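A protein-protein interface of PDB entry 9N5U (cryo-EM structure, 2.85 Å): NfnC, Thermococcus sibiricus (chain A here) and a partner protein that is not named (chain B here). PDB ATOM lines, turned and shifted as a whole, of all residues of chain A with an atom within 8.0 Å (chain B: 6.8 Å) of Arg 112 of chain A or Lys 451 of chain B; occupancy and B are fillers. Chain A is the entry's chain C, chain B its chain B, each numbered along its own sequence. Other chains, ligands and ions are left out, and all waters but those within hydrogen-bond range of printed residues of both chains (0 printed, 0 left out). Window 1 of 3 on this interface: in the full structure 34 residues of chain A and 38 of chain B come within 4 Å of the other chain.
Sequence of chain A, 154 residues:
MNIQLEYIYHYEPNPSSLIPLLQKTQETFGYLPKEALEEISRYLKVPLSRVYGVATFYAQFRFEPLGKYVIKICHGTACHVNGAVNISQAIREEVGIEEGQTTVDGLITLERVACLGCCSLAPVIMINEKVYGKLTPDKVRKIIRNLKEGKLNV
NH1 of Arg 112 of chain A is in salt-bridge range of OD2 of Asp 447 of chain B (3.9 Å).
NZ of Lys 451 of chain B lies within salt-bridge range of OD1 of Asp 447 of chain B. The backbone carbonyl oxygen (O) of Val 113 of chain A sits at hydrogen-bond distance from the backbone NH (N) of His 75 of chain A (3.0 Å). N of Gly 76 of chain A sits at hydrogen-bond distance from O of Ala 114 of chain A. The backbone NH (N) of Gly 76 of chain A sits close to the side-chain sulfur (SG) of Cys 74 of chain A. NE of Arg 112 of chain A is in hydrogen-bond range of ND1 of His 75 of chain A, at 3.2 Å. The guanidinium group (NE) of Arg 112 of chain A is in salt-bridge range of the side-chain carboxylate (OE1) of Glu 99 of chain A (3.4 Å).
CE1 of Phe 57 of chain A touches CB of Cys 454 of chain B, at 3.8 Å. Phe 444 of chain B touches His 75 of chain A. C of Gly 76 of chain A touches CZ of Phe 444 of chain B (3.8 Å). His 80 of chain A touches Phe 444 of chain B (ND1 to CD1, 3.6 Å). NH1 of Arg 112 of chain A touches CE of Lys 451 of chain B (3.8 Å).
Printed residues of chain B within 4 Å of Phe 57 of chain A: Cys 454 (3.8 Å). Of the printed residues of chain B, His 75 of chain A touches Phe 444 (3.2 Å). Printed residues of chain B within 4 Å of Gly 76 of chain A: Phe 444. Val 85 of chain A touches none of the printed residues of chain B. Thr 109 of chain A touches none of the printed residues of chain B. Of the printed residues of chain A, Phe 444 of chain B touches His 75 (3.2 Å), Gly 76 (3.8 Å) and His 80 (3.6 Å). Of chain A, only Arg 112 comes within 4 Å of Lys 451 of chain B. Of the printed residues of chain A, Cys 454 of chain B touches Phe 57. The nearest residue of chain B that does not touch Arg 112 of chain A is Phe 448 of chain B (6.1 Å).
Hydrophobic or aromatic side chains of chain A within 4 Å of the printed part of chain B: Phe 57 and His 80. Hydrophobic or aromatic side chains of chain B within 4 Å of the printed part of chain A: Phe 444. Among the printed residues, 6 pairs touch across the chains.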
ATOM      1  N   PHE A  57      19.197  14.361  35.838  1.00  0.00           N
ATOM      2  CA  PHE A  57      19.035  15.810  35.939  1.00  0.00           C
ATOM      3  C   PHE A  57      18.495  16.415  34.645  1.00  0.00           C
ATOM      4  O   PHE A  57      17.668  17.333  34.683  1.00  0.00           O
ATOM      5  CB  PHE A  57      20.364  16.461  36.314  1.00  0.00           C
ATOM      6  CG  PHE A  57      20.253  17.922  36.637  1.00  0.00           C
ATOM      7  CD1 PHE A  57      19.896  18.336  37.904  1.00  0.00           C
ATOM      8  CD2 PHE A  57      20.520  18.881  35.678  1.00  0.00           C
ATOM      9  CE1 PHE A  57      19.799  19.674  38.207  1.00  0.00           C
ATOM     10  CE2 PHE A  57      20.420  20.219  35.976  1.00  0.00           C
ATOM     11  CZ  PHE A  57      20.061  20.616  37.243  1.00  0.00           C
ATOM     12  N   ALA A  59      16.500  16.614  31.049  1.00  0.00           N
ATOM     13  CA  ALA A  59      15.297  16.050  30.451  1.00  0.00           C
ATOM     14  C   ALA A  59      15.555  15.392  29.104  1.00  0.00           C
ATOM     15  O   ALA A  59      14.673  14.691  28.601  1.00  0.00           O
ATOM     16  CB  ALA A  59      14.229  17.133  30.296  1.00  0.00           C
ATOM     17  N   VAL A  70       7.832  10.910  17.053  1.00  0.00           N
ATOM     18  CA  VAL A  70       7.983  11.735  18.240  1.00  0.00           C
ATOM     19  C   VAL A  70       7.217  13.024  17.997  1.00  0.00           C
ATOM     20  O   VAL A  70       7.515  13.765  17.054  1.00  0.00           O
ATOM     21  CB  VAL A  70       9.461  12.011  18.552  1.00  0.00           C
ATOM     22  CG1 VAL A  70       9.591  12.777  19.851  1.00  0.00           C
ATOM     23  CG2 VAL A  70      10.236  10.714  18.627  1.00  0.00           C
ATOM     24  N   ILE A  71       6.218  13.286  18.830  1.00  0.00           N
ATOM     25  CA  ILE A  71       5.435  14.509  18.743  1.00  0.00           C
ATOM     26  C   ILE A  71       5.964  15.474  19.789  1.00  0.00           C
ATOM     27  O   ILE A  71       6.020  15.143  20.979  1.00  0.00           O
ATOM     28  CB  ILE A  71       3.939  14.242  18.945  1.00  0.00           C
ATOM     29  CG1 ILE A  71       3.469  13.140  18.005  1.00  0.00           C
ATOM     30  CG2 ILE A  71       3.146  15.509  18.706  1.00  0.00           C
ATOM     31  CD1 ILE A  71       2.005  12.869  18.098  1.00  0.00           C
ATOM     32  N   LYS A  72       6.365  16.655  19.348  1.00  0.00           N
ATOM     33  CA  LYS A  72       6.894  17.687  20.228  1.00  0.00           C
ATOM     34  C   LYS A  72       5.882  18.821  20.286  1.00  0.00           C
ATOM     35  O   LYS A  72       5.716  19.562  19.312  1.00  0.00           O
ATOM     36  CB  LYS A  72       8.252  18.179  19.741  1.00  0.00           C
ATOM     37  CG  LYS A  72       9.358  17.152  19.863  1.00  0.00           C
ATOM     38  CD  LYS A  72      10.680  17.725  19.399  1.00  0.00           C
ATOM     39  CE  LYS A  72      11.803  16.725  19.558  1.00  0.00           C
ATOM     40  NZ  LYS A  72      11.977  16.319  20.978  1.00  0.00           N
ATOM     41  N   ILE A  73       5.205  18.949  21.420  1.00  0.00           N
ATOM     42  CA  ILE A  73       4.279  20.049  21.650  1.00  0.00           C
ATOM     43  C   ILE A  73       5.066  21.198  22.256  1.00  0.00           C
ATOM     44  O   ILE A  73       5.659  21.058  23.330  1.00  0.00           O
ATOM     45  CB  ILE A  73       3.125  19.631  22.572  1.00  0.00           C
ATOM     46  CG1 ILE A  73       2.506  18.318  22.107  1.00  0.00           C
ATOM     47  CG2 ILE A  73       2.067  20.717  22.611  1.00  0.00           C
ATOM     48  CD1 ILE A  73       1.285  17.935  22.898  1.00  0.00           C
ATOM     49  N   CYS A  74       5.083  22.332  21.569  1.00  0.00           N
ATOM     50  CA  CYS A  74       5.799  23.493  22.071  1.00  0.00           C
ATOM     51  C   CYS A  74       4.929  24.216  23.087  1.00  0.00           C
ATOM     52  O   CYS A  74       3.841  24.695  22.754  1.00  0.00           O
ATOM     53  CB  CYS A  74       6.187  24.428  20.932  1.00  0.00           C
ATOM     54  SG  CYS A  74       7.177  25.821  21.480  1.00  0.00           S
ATOM     55  N   HIS A  75       5.400  24.285  24.324  1.00  0.00           N
ATOM     56  CA  HIS A  75       4.714  25.008  25.386  1.00  0.00           C
ATOM     57  C   HIS A  75       5.496  26.249  25.799  1.00  0.00           C
ATOM     58  O   HIS A  75       5.592  26.582  26.979  1.00  0.00           O
ATOM     59  CB  HIS A  75       4.456  24.102  26.584  1.00  0.00           C
ATOM     60  CG  HIS A  75       3.274  23.204  26.411  1.00  0.00           C
ATOM     61  ND1 HIS A  75       3.390  21.838  26.274  1.00  0.00           N
ATOM     62  CD2 HIS A  75       1.950  23.477  26.341  1.00  0.00           C
ATOM     63  CE1 HIS A  75       2.188  21.309  26.135  1.00  0.00           C
ATOM     64  NE2 HIS A  75       1.297  22.282  26.170  1.00  0.00           N
ATOM     65  N   GLY A  76       6.071  26.939  24.823  1.00  0.00           N
ATOM     66  CA  GLY A  76       6.648  28.238  25.078  1.00  0.00           C
ATOM     67  C   GLY A  76       5.568  29.269  25.298  1.00  0.00           C
ATOM     68  O   GLY A  76       4.373  29.002  25.169  1.00  0.00           O
ATOM     69  N   HIS A  80       1.750  29.053  24.172  1.00  0.00           N
ATOM     70  CA  HIS A  80       0.779  28.941  25.252  1.00  0.00           C
ATOM     71  C   HIS A  80      -0.299  30.009  25.138  1.00  0.00           C
ATOM     72  O   HIS A  80      -1.488  29.723  25.313  1.00  0.00           O
ATOM     73  CB  HIS A  80       1.474  29.031  26.608  1.00  0.00           C
ATOM     74  CG  HIS A  80       0.542  28.879  27.765  1.00  0.00           C
ATOM     75  ND1 HIS A  80       0.111  27.650  28.215  1.00  0.00           N
ATOM     76  CD2 HIS A  80      -0.060  29.800  28.552  1.00  0.00           C
ATOM     77  CE1 HIS A  80      -0.707  27.822  29.238  1.00  0.00           C
ATOM     78  NE2 HIS A  80      -0.828  29.117  29.461  1.00  0.00           N
ATOM     79  N   ALA A  84      -1.807  26.517  23.295  1.00  0.00           N
ATOM     80  CA  ALA A  84      -1.065  25.264  23.384  1.00  0.00           C
ATOM     81  C   ALA A  84      -1.788  24.236  24.242  1.00  0.00           C
ATOM     82  O   ALA A  84      -1.640  23.033  24.016  1.00  0.00           O
ATOM     83  CB  ALA A  84       0.341  25.511  23.928  1.00  0.00           C
ATOM     84  N   VAL A  85      -2.563  24.683  25.230  1.00  0.00           N
ATOM     85  CA  VAL A  85      -3.285  23.744  26.083  1.00  0.00           C
ATOM     86  C   VAL A  85      -4.362  23.015  25.288  1.00  0.00           C
ATOM     87  O   VAL A  85      -4.539  21.802  25.432  1.00  0.00           O
ATOM     88  CB  VAL A  85      -3.867  24.473  27.307  1.00  0.00           C
ATOM     89  CG1 VAL A  85      -4.598  23.498  28.205  1.00  0.00           C
ATOM     90  CG2 VAL A  85      -2.763  25.163  28.076  1.00  0.00           C
ATOM     91  N   SER A  88      -2.625  20.524  22.945  1.00  0.00           N
ATOM     92  CA  SER A  88      -2.132  19.388  23.716  1.00  0.00           C
ATOM     93  C   SER A  88      -3.274  18.495  24.174  1.00  0.00           C
ATOM     94  O   SER A  88      -3.121  17.274  24.226  1.00  0.00           O
ATOM     95  CB  SER A  88      -1.314  19.863  24.915  1.00  0.00           C
ATOM     96  OG  SER A  88      -2.128  20.547  25.849  1.00  0.00           O
ATOM     97  N   ARG A  92      -3.478  14.621  23.205  1.00  0.00           N
ATOM     98  CA  ARG A  92      -3.602  13.610  24.247  1.00  0.00           C
ATOM     99  C   ARG A  92      -4.881  12.800  24.092  1.00  0.00           C
ATOM    100  O   ARG A  92      -4.896  11.598  24.374  1.00  0.00           O
ATOM    101  CB  ARG A  92      -3.552  14.268  25.624  1.00  0.00           C
ATOM    102  CG  ARG A  92      -2.170  14.703  26.061  1.00  0.00           C
ATOM    103  CD  ARG A  92      -2.265  15.781  27.116  1.00  0.00           C
ATOM    104  NE  ARG A  92      -3.267  15.459  28.121  1.00  0.00           N
ATOM    105  CZ  ARG A  92      -3.713  16.313  29.031  1.00  0.00           C
ATOM    106  NH1 ARG A  92      -3.268  17.556  29.089  1.00  0.00           N
ATOM    107  NH2 ARG A  92      -4.632  15.910  29.903  1.00  0.00           N
ATOM    108  N   GLU A  99       1.555  13.583  28.141  1.00  0.00           N
ATOM    109  CA  GLU A  99       2.851  14.042  27.667  1.00  0.00           C
ATOM    110  C   GLU A  99       3.968  13.395  28.477  1.00  0.00           C
ATOM    111  O   GLU A  99       3.882  13.281  29.702  1.00  0.00           O
ATOM    112  CB  GLU A  99       2.934  15.563  27.759  1.00  0.00           C
ATOM    113  CG  GLU A  99       1.759  16.278  27.110  1.00  0.00           C
ATOM    114  CD  GLU A  99       1.725  17.763  27.423  1.00  0.00           C
ATOM    115  OE1 GLU A  99       2.728  18.283  27.954  1.00  0.00           O
ATOM    116  OE2 GLU A  99       0.691  18.408  27.141  1.00  0.00           O
ATOM    117  N   GLY A 100       5.018  12.966  27.786  1.00  0.00           N
ATOM    118  CA  GLY A 100       6.107  12.261  28.427  1.00  0.00           C
ATOM    119  C   GLY A 100       5.949  10.761  28.496  1.00  0.00           C
ATOM    120  O   GLY A 100       6.655  10.112  29.274  1.00  0.00           O
ATOM    121  N   GLN A 101       5.048  10.185  27.704  1.00  0.00           N
ATOM    122  CA  GLN A 101       4.774   8.758  27.729  1.00  0.00           C
ATOM    123  C   GLN A 101       4.883   8.187  26.323  1.00  0.00           C
ATOM    124  O   GLN A 101       4.777   8.904  25.325  1.00  0.00           O
ATOM    125  CB  GLN A 101       3.383   8.466  28.297  1.00  0.00           C
ATOM    126  CG  GLN A 101       3.161   8.992  29.695  1.00  0.00           C
ATOM    127  CD  GLN A 101       1.714   8.891  30.125  1.00  0.00           C
ATOM    128  OE1 GLN A 101       0.823   8.694  29.299  1.00  0.00           O
ATOM    129  NE2 GLN A 101       1.471   9.022  31.423  1.00  0.00           N
ATOM    130  N   THR A 109       5.453   8.698  20.478  1.00  0.00           N
ATOM    131  CA  THR A 109       6.007   9.197  21.727  1.00  0.00           C
ATOM    132  C   THR A 109       5.666  10.675  21.845  1.00  0.00           C
ATOM    133  O   THR A 109       5.910  11.447  20.914  1.00  0.00           O
ATOM    134  CB  THR A 109       7.520   8.992  21.789  1.00  0.00           C
ATOM    135  OG1 THR A 109       7.812   7.592  21.739  1.00  0.00           O
ATOM    136  CG2 THR A 109       8.081   9.570  23.074  1.00  0.00           C
ATOM    137  N   LEU A 110       5.098  11.061  22.980  1.00  0.00           N
ATOM    138  CA  LEU A 110       4.576  12.406  23.182  1.00  0.00           C
ATOM    139  C   LEU A 110       5.507  13.167  24.115  1.00  0.00           C
ATOM    140  O   LEU A 110       5.786  12.708  25.227  1.00  0.00           O
ATOM    141  CB  LEU A 110       3.158  12.343  23.746  1.00  0.00           C
ATOM    142  CG  LEU A 110       2.159  13.376  23.238  1.00  0.00           C
ATOM    143  CD1 LEU A 110       0.753  12.959  23.600  1.00  0.00           C
ATOM    144  CD2 LEU A 110       2.474  14.721  23.838  1.00  0.00           C
ATOM    145  N   GLU A 111       5.975  14.330  23.666  1.00  0.00           N
ATOM    146  CA  GLU A 111       6.964  15.114  24.389  1.00  0.00           C
ATOM    147  C   GLU A 111       6.550  16.579  24.431  1.00  0.00           C
ATOM    148  O   GLU A 111       5.774  17.054  23.600  1.00  0.00           O
ATOM    149  CB  GLU A 111       8.354  14.998  23.749  1.00  0.00           C
ATOM    150  CG  GLU A 111       8.916  13.595  23.732  1.00  0.00           C
ATOM    151  CD  GLU A 111      10.328  13.548  23.189  1.00  0.00           C
ATOM    152  OE1 GLU A 111      10.864  14.621  22.841  1.00  0.00           O
ATOM    153  OE2 GLU A 111      10.900  12.442  23.109  1.00  0.00           O
ATOM    154  N   ARG A 112       7.085  17.290  25.419  1.00  0.00           N
ATOM    155  CA  ARG A 112       6.895  18.727  25.567  1.00  0.00           C
ATOM    156  C   ARG A 112       8.237  19.423  25.400  1.00  0.00           C
ATOM    157  O   ARG A 112       9.229  19.017  26.013  1.00  0.00           O
ATOM    158  CB  ARG A 112       6.292  19.073  26.930  1.00  0.00           C
ATOM    159  CG  ARG A 112       6.424  20.537  27.290  1.00  0.00           C
ATOM    160  CD  ARG A 112       6.116  20.797  28.749  1.00  0.00           C
ATOM    161  NE  ARG A 112       4.684  20.828  29.010  1.00  0.00           N
ATOM    162  CZ  ARG A 112       4.140  21.321  30.112  1.00  0.00           C
ATOM    163  NH1 ARG A 112       4.882  21.843  31.075  1.00  0.00           N
ATOM    164  NH2 ARG A 112       2.819  21.293  30.253  1.00  0.00           N
ATOM    165  N   VAL A 113       8.268  20.467  24.575  1.00  0.00           N
ATOM    166  CA  VAL A 113       9.500  21.193  24.306  1.00  0.00           C
ATOM    167  C   VAL A 113       9.293  22.666  24.627  1.00  0.00           C
ATOM    168  O   VAL A 113       8.169  23.153  24.753  1.00  0.00           O
ATOM    169  CB  VAL A 113       9.978  21.014  22.852  1.00  0.00           C
ATOM    170  CG1 VAL A 113      10.291  19.556  22.581  1.00  0.00           C
ATOM    171  CG2 VAL A 113       8.936  21.531  21.884  1.00  0.00           C
ATOM    172  N   ALA A 114      10.413  23.376  24.765  1.00  0.00           N
ATOM    173  CA  ALA A 114      10.372  24.773  25.182  1.00  0.00           C
ATOM    174  C   ALA A 114      10.049  25.694  24.013  1.00  0.00           C
ATOM    175  O   ALA A 114       9.036  26.399  24.026  1.00  0.00           O
ATOM    176  CB  ALA A 114      11.703  25.166  25.824  1.00  0.00           C
ATOM    177  N   CYS A 115      10.900  25.704  22.994  1.00  0.00           N
ATOM    178  CA  CYS A 115      10.688  26.565  21.844  1.00  0.00           C
ATOM    179  C   CYS A 115      11.292  25.900  20.619  1.00  0.00           C
ATOM    180  O   CYS A 115      12.214  25.088  20.721  1.00  0.00           O
ATOM    181  CB  CYS A 115      11.297  27.954  22.058  1.00  0.00           C
ATOM    182  SG  CYS A 115      10.739  29.224  20.901  1.00  0.00           S
ATOM    183  N   LEU A 116      10.761  26.258  19.456  1.00  0.00           N
ATOM    184  CA  LEU A 116      11.244  25.728  18.193  1.00  0.00           C
ATOM    185  C   LEU A 116      11.694  26.816  17.230  1.00  0.00           C
ATOM    186  O   LEU A 116      12.170  26.495  16.136  1.00  0.00           O
ATOM    187  CB  LEU A 116      10.164  24.860  17.536  1.00  0.00           C
ATOM    188  CG  LEU A 116       9.682  23.689  18.394  1.00  0.00           C
ATOM    189  CD1 LEU A 116       8.578  22.919  17.700  1.00  0.00           C
ATOM    190  CD2 LEU A 116      10.842  22.775  18.735  1.00  0.00           C
ATOM    191  N   PHE B 444       1.321  29.653  34.334  1.00  0.00           N
ATOM    192  CA  PHE B 444       2.208  29.055  33.338  1.00  0.00           C
ATOM    193  C   PHE B 444       3.673  29.305  33.677  1.00  0.00           C
ATOM    194  O   PHE B 444       4.507  28.390  33.605  1.00  0.00           O
ATOM    195  CB  PHE B 444       1.862  29.613  31.956  1.00  0.00           C
ATOM    196  CG  PHE B 444       2.911  29.367  30.913  1.00  0.00           C
ATOM    197  CD1 PHE B 444       2.979  28.156  30.255  1.00  0.00           C
ATOM    198  CD2 PHE B 444       3.808  30.360  30.570  1.00  0.00           C
ATOM    199  CE1 PHE B 444       3.934  27.934  29.294  1.00  0.00           C
ATOM    200  CE2 PHE B 444       4.765  30.140  29.613  1.00  0.00           C
ATOM    201  CZ  PHE B 444       4.829  28.926  28.974  1.00  0.00           C
ATOM    202  N   LEU B 446       4.975  30.020  36.652  1.00  0.00           N
ATOM    203  CA  LEU B 446       5.340  29.281  37.855  1.00  0.00           C
ATOM    204  C   LEU B 446       5.421  27.782  37.596  1.00  0.00           C
ATOM    205  O   LEU B 446       6.224  27.094  38.226  1.00  0.00           O
ATOM    206  CB  LEU B 446       4.350  29.582  38.977  1.00  0.00           C
ATOM    207  CG  LEU B 446       4.847  30.559  40.044  1.00  0.00           C
ATOM    208  CD1 LEU B 446       5.906  29.904  40.910  1.00  0.00           C
ATOM    209  CD2 LEU B 446       5.393  31.817  39.403  1.00  0.00           C
ATOM    210  N   ASP B 447       4.614  27.264  36.670  1.00  0.00           N
ATOM    211  CA  ASP B 447       4.721  25.867  36.267  1.00  0.00           C
ATOM    212  C   ASP B 447       6.071  25.592  35.620  1.00  0.00           C
ATOM    213  O   ASP B 447       6.740  24.598  35.935  1.00  0.00           O
ATOM    214  CB  ASP B 447       3.576  25.536  35.308  1.00  0.00           C
ATOM    215  CG  ASP B 447       3.575  24.094  34.865  1.00  0.00           C
ATOM    216  OD1 ASP B 447       4.176  23.247  35.557  1.00  0.00           O
ATOM    217  OD2 ASP B 447       2.964  23.808  33.815  1.00  0.00           O
ATOM    218  N   PHE B 448       6.494  26.482  34.720  1.00  0.00           N
ATOM    219  CA  PHE B 448       7.808  26.334  34.106  1.00  0.00           C
ATOM    220  C   PHE B 448       8.913  26.416  35.152  1.00  0.00           C
ATOM    221  O   PHE B 448       9.864  25.627  35.123  1.00  0.00           O
ATOM    222  CB  PHE B 448       8.005  27.393  33.023  1.00  0.00           C
ATOM    223  CG  PHE B 448       9.319  27.292  32.311  1.00  0.00           C
ATOM    224  CD1 PHE B 448       9.535  26.307  31.368  1.00  0.00           C
ATOM    225  CD2 PHE B 448      10.338  28.184  32.582  1.00  0.00           C
ATOM    226  CE1 PHE B 448      10.742  26.213  30.715  1.00  0.00           C
ATOM    227  CE2 PHE B 448      11.543  28.094  31.929  1.00  0.00           C
ATOM    228  CZ  PHE B 448      11.745  27.107  30.995  1.00  0.00           C
ATOM    229  N   THR B 449       8.791  27.351  36.097  1.00  0.00           N
ATOM    230  CA  THR B 449       9.793  27.476  37.152  1.00  0.00           C
ATOM    231  C   THR B 449       9.853  26.226  38.024  1.00  0.00           C
ATOM    232  O   THR B 449      10.940  25.783  38.411  1.00  0.00           O
ATOM    233  CB  THR B 449       9.498  28.706  38.006  1.00  0.00           C
ATOM    234  OG1 THR B 449       9.574  29.886  37.197  1.00  0.00           O
ATOM    235  CG2 THR B 449      10.500  28.805  39.124  1.00  0.00           C
ATOM    236  N   VAL B 450       8.692  25.648  38.345  1.00  0.00           N
ATOM    237  CA  VAL B 450       8.646  24.422  39.137  1.00  0.00           C
ATOM    238  C   VAL B 450       9.334  23.284  38.397  1.00  0.00           C
ATOM    239  O   VAL B 450      10.091  22.506  38.992  1.00  0.00           O
ATOM    240  CB  VAL B 450       7.187  24.074  39.496  1.00  0.00           C
ATOM    241  CG1 VAL B 450       7.059  22.630  39.944  1.00  0.00           C
ATOM    242  CG2 VAL B 450       6.683  24.988  40.586  1.00  0.00           C
ATOM    243  N   LYS B 451       9.089  23.170  37.088  1.00  0.00           N
ATOM    244  CA  LYS B 451       9.743  22.128  36.300  1.00  0.00           C
ATOM    245  C   LYS B 451      11.256  22.316  36.250  1.00  0.00           C
ATOM    246  O   LYS B 451      12.014  21.348  36.372  1.00  0.00           O
ATOM    247  CB  LYS B 451       9.177  22.109  34.881  1.00  0.00           C
ATOM    248  CG  LYS B 451       8.259  20.947  34.570  1.00  0.00           C
ATOM    249  CD  LYS B 451       6.834  21.243  34.967  1.00  0.00           C
ATOM    250  CE  LYS B 451       5.885  20.218  34.384  1.00  0.00           C
ATOM    251  NZ  LYS B 451       4.478  20.477  34.788  1.00  0.00           N
ATOM    252  N   GLU B 452      11.715  23.554  36.069  1.00  0.00           N
ATOM    253  CA  GLU B 452      13.110  23.817  35.739  1.00  0.00           C
ATOM    254  C   GLU B 452      14.002  24.038  36.950  1.00  0.00           C
ATOM    255  O   GLU B 452      15.218  24.172  36.780  1.00  0.00           O
ATOM    256  CB  GLU B 452      13.211  25.035  34.821  1.00  0.00           C
ATOM    257  CG  GLU B 452      12.577  24.820  33.469  1.00  0.00           C
ATOM    258  CD  GLU B 452      13.295  23.770  32.646  1.00  0.00           C
ATOM    259  OE1 GLU B 452      14.513  23.582  32.844  1.00  0.00           O
ATOM    260  OE2 GLU B 452      12.639  23.130  31.799  1.00  0.00           O
ATOM    261  N   SER B 453      13.441  24.087  38.153  1.00  0.00           N
ATOM    262  CA  SER B 453      14.253  24.252  39.348  1.00  0.00           C
ATOM    263  C   SER B 453      15.158  23.043  39.542  1.00  0.00           C
ATOM    264  O   SER B 453      14.771  21.909  39.257  1.00  0.00           O
ATOM    265  CB  SER B 453      13.354  24.444  40.568  1.00  0.00           C
ATOM    266  OG  SER B 453      14.099  24.362  41.766  1.00  0.00           O
ATOM    267  N   CYS B 454      16.377  23.289  40.017  1.00  0.00           N
ATOM    268  CA  CYS B 454      17.301  22.191  40.262  1.00  0.00           C
ATOM    269  C   CYS B 454      17.016  21.457  41.564  1.00  0.00           C
ATOM    270  O   CYS B 454      17.584  20.383  41.785  1.00  0.00           O
ATOM    271  CB  CYS B 454      18.746  22.696  40.261  1.00  0.00           C
ATOM    272  SG  CYS B 454      19.224  23.675  41.691  1.00  0.00           S
ATOM    273  N   THR B 464       8.238  27.523  45.196  1.00  0.00           N
ATOM    274  CA  THR B 464       7.675  27.605  43.854  1.00  0.00           C
ATOM    275  C   THR B 464       6.537  26.610  43.678  1.00  0.00           C
ATOM    276  O   THR B 464       5.520  26.926  43.054  1.00  0.00           O
ATOM    277  CB  THR B 464       8.763  27.394  42.802  1.00  0.00           C
ATOM    278  OG1 THR B 464       9.514  26.215  43.107  1.00  0.00           O
ATOM    279  CG2 THR B 464       9.692  28.592  42.769  1.00  0.00           C
ATOM    280  N   TRP B 468       2.721  27.703  42.951  1.00  0.00           N
ATOM    281  CA  TRP B 468       1.997  27.146  41.815  1.00  0.00           C
ATOM    282  C   TRP B 468       0.723  26.439  42.262  1.00  0.00           C
ATOM    283  O   TRP B 468      -0.295  26.491  41.567  1.00  0.00           O
ATOM    284  CB  TRP B 468       2.886  26.191  41.024  1.00  0.00           C
ATOM    285  CG  TRP B 468       2.145  25.563  39.901  1.00  0.00           C
ATOM    286  CD1 TRP B 468       1.916  26.100  38.673  1.00  0.00           C
ATOM    287  CD2 TRP B 468       1.492  24.291  39.912  1.00  0.00           C
ATOM    288  NE1 TRP B 468       1.172  25.237  37.910  1.00  0.00           N
ATOM    289  CE2 TRP B 468       0.898  24.117  38.649  1.00  0.00           C
ATOM    290  CE3 TRP B 468       1.356  23.279  40.865  1.00  0.00           C
ATOM    291  CZ2 TRP B 468       0.183  22.976  38.315  1.00  0.00           C
ATOM    292  CZ3 TRP B 468       0.645  22.151  40.533  1.00  0.00           C
ATOM    293  CH2 TRP B 468       0.068  22.005  39.269  1.00  0.00           C
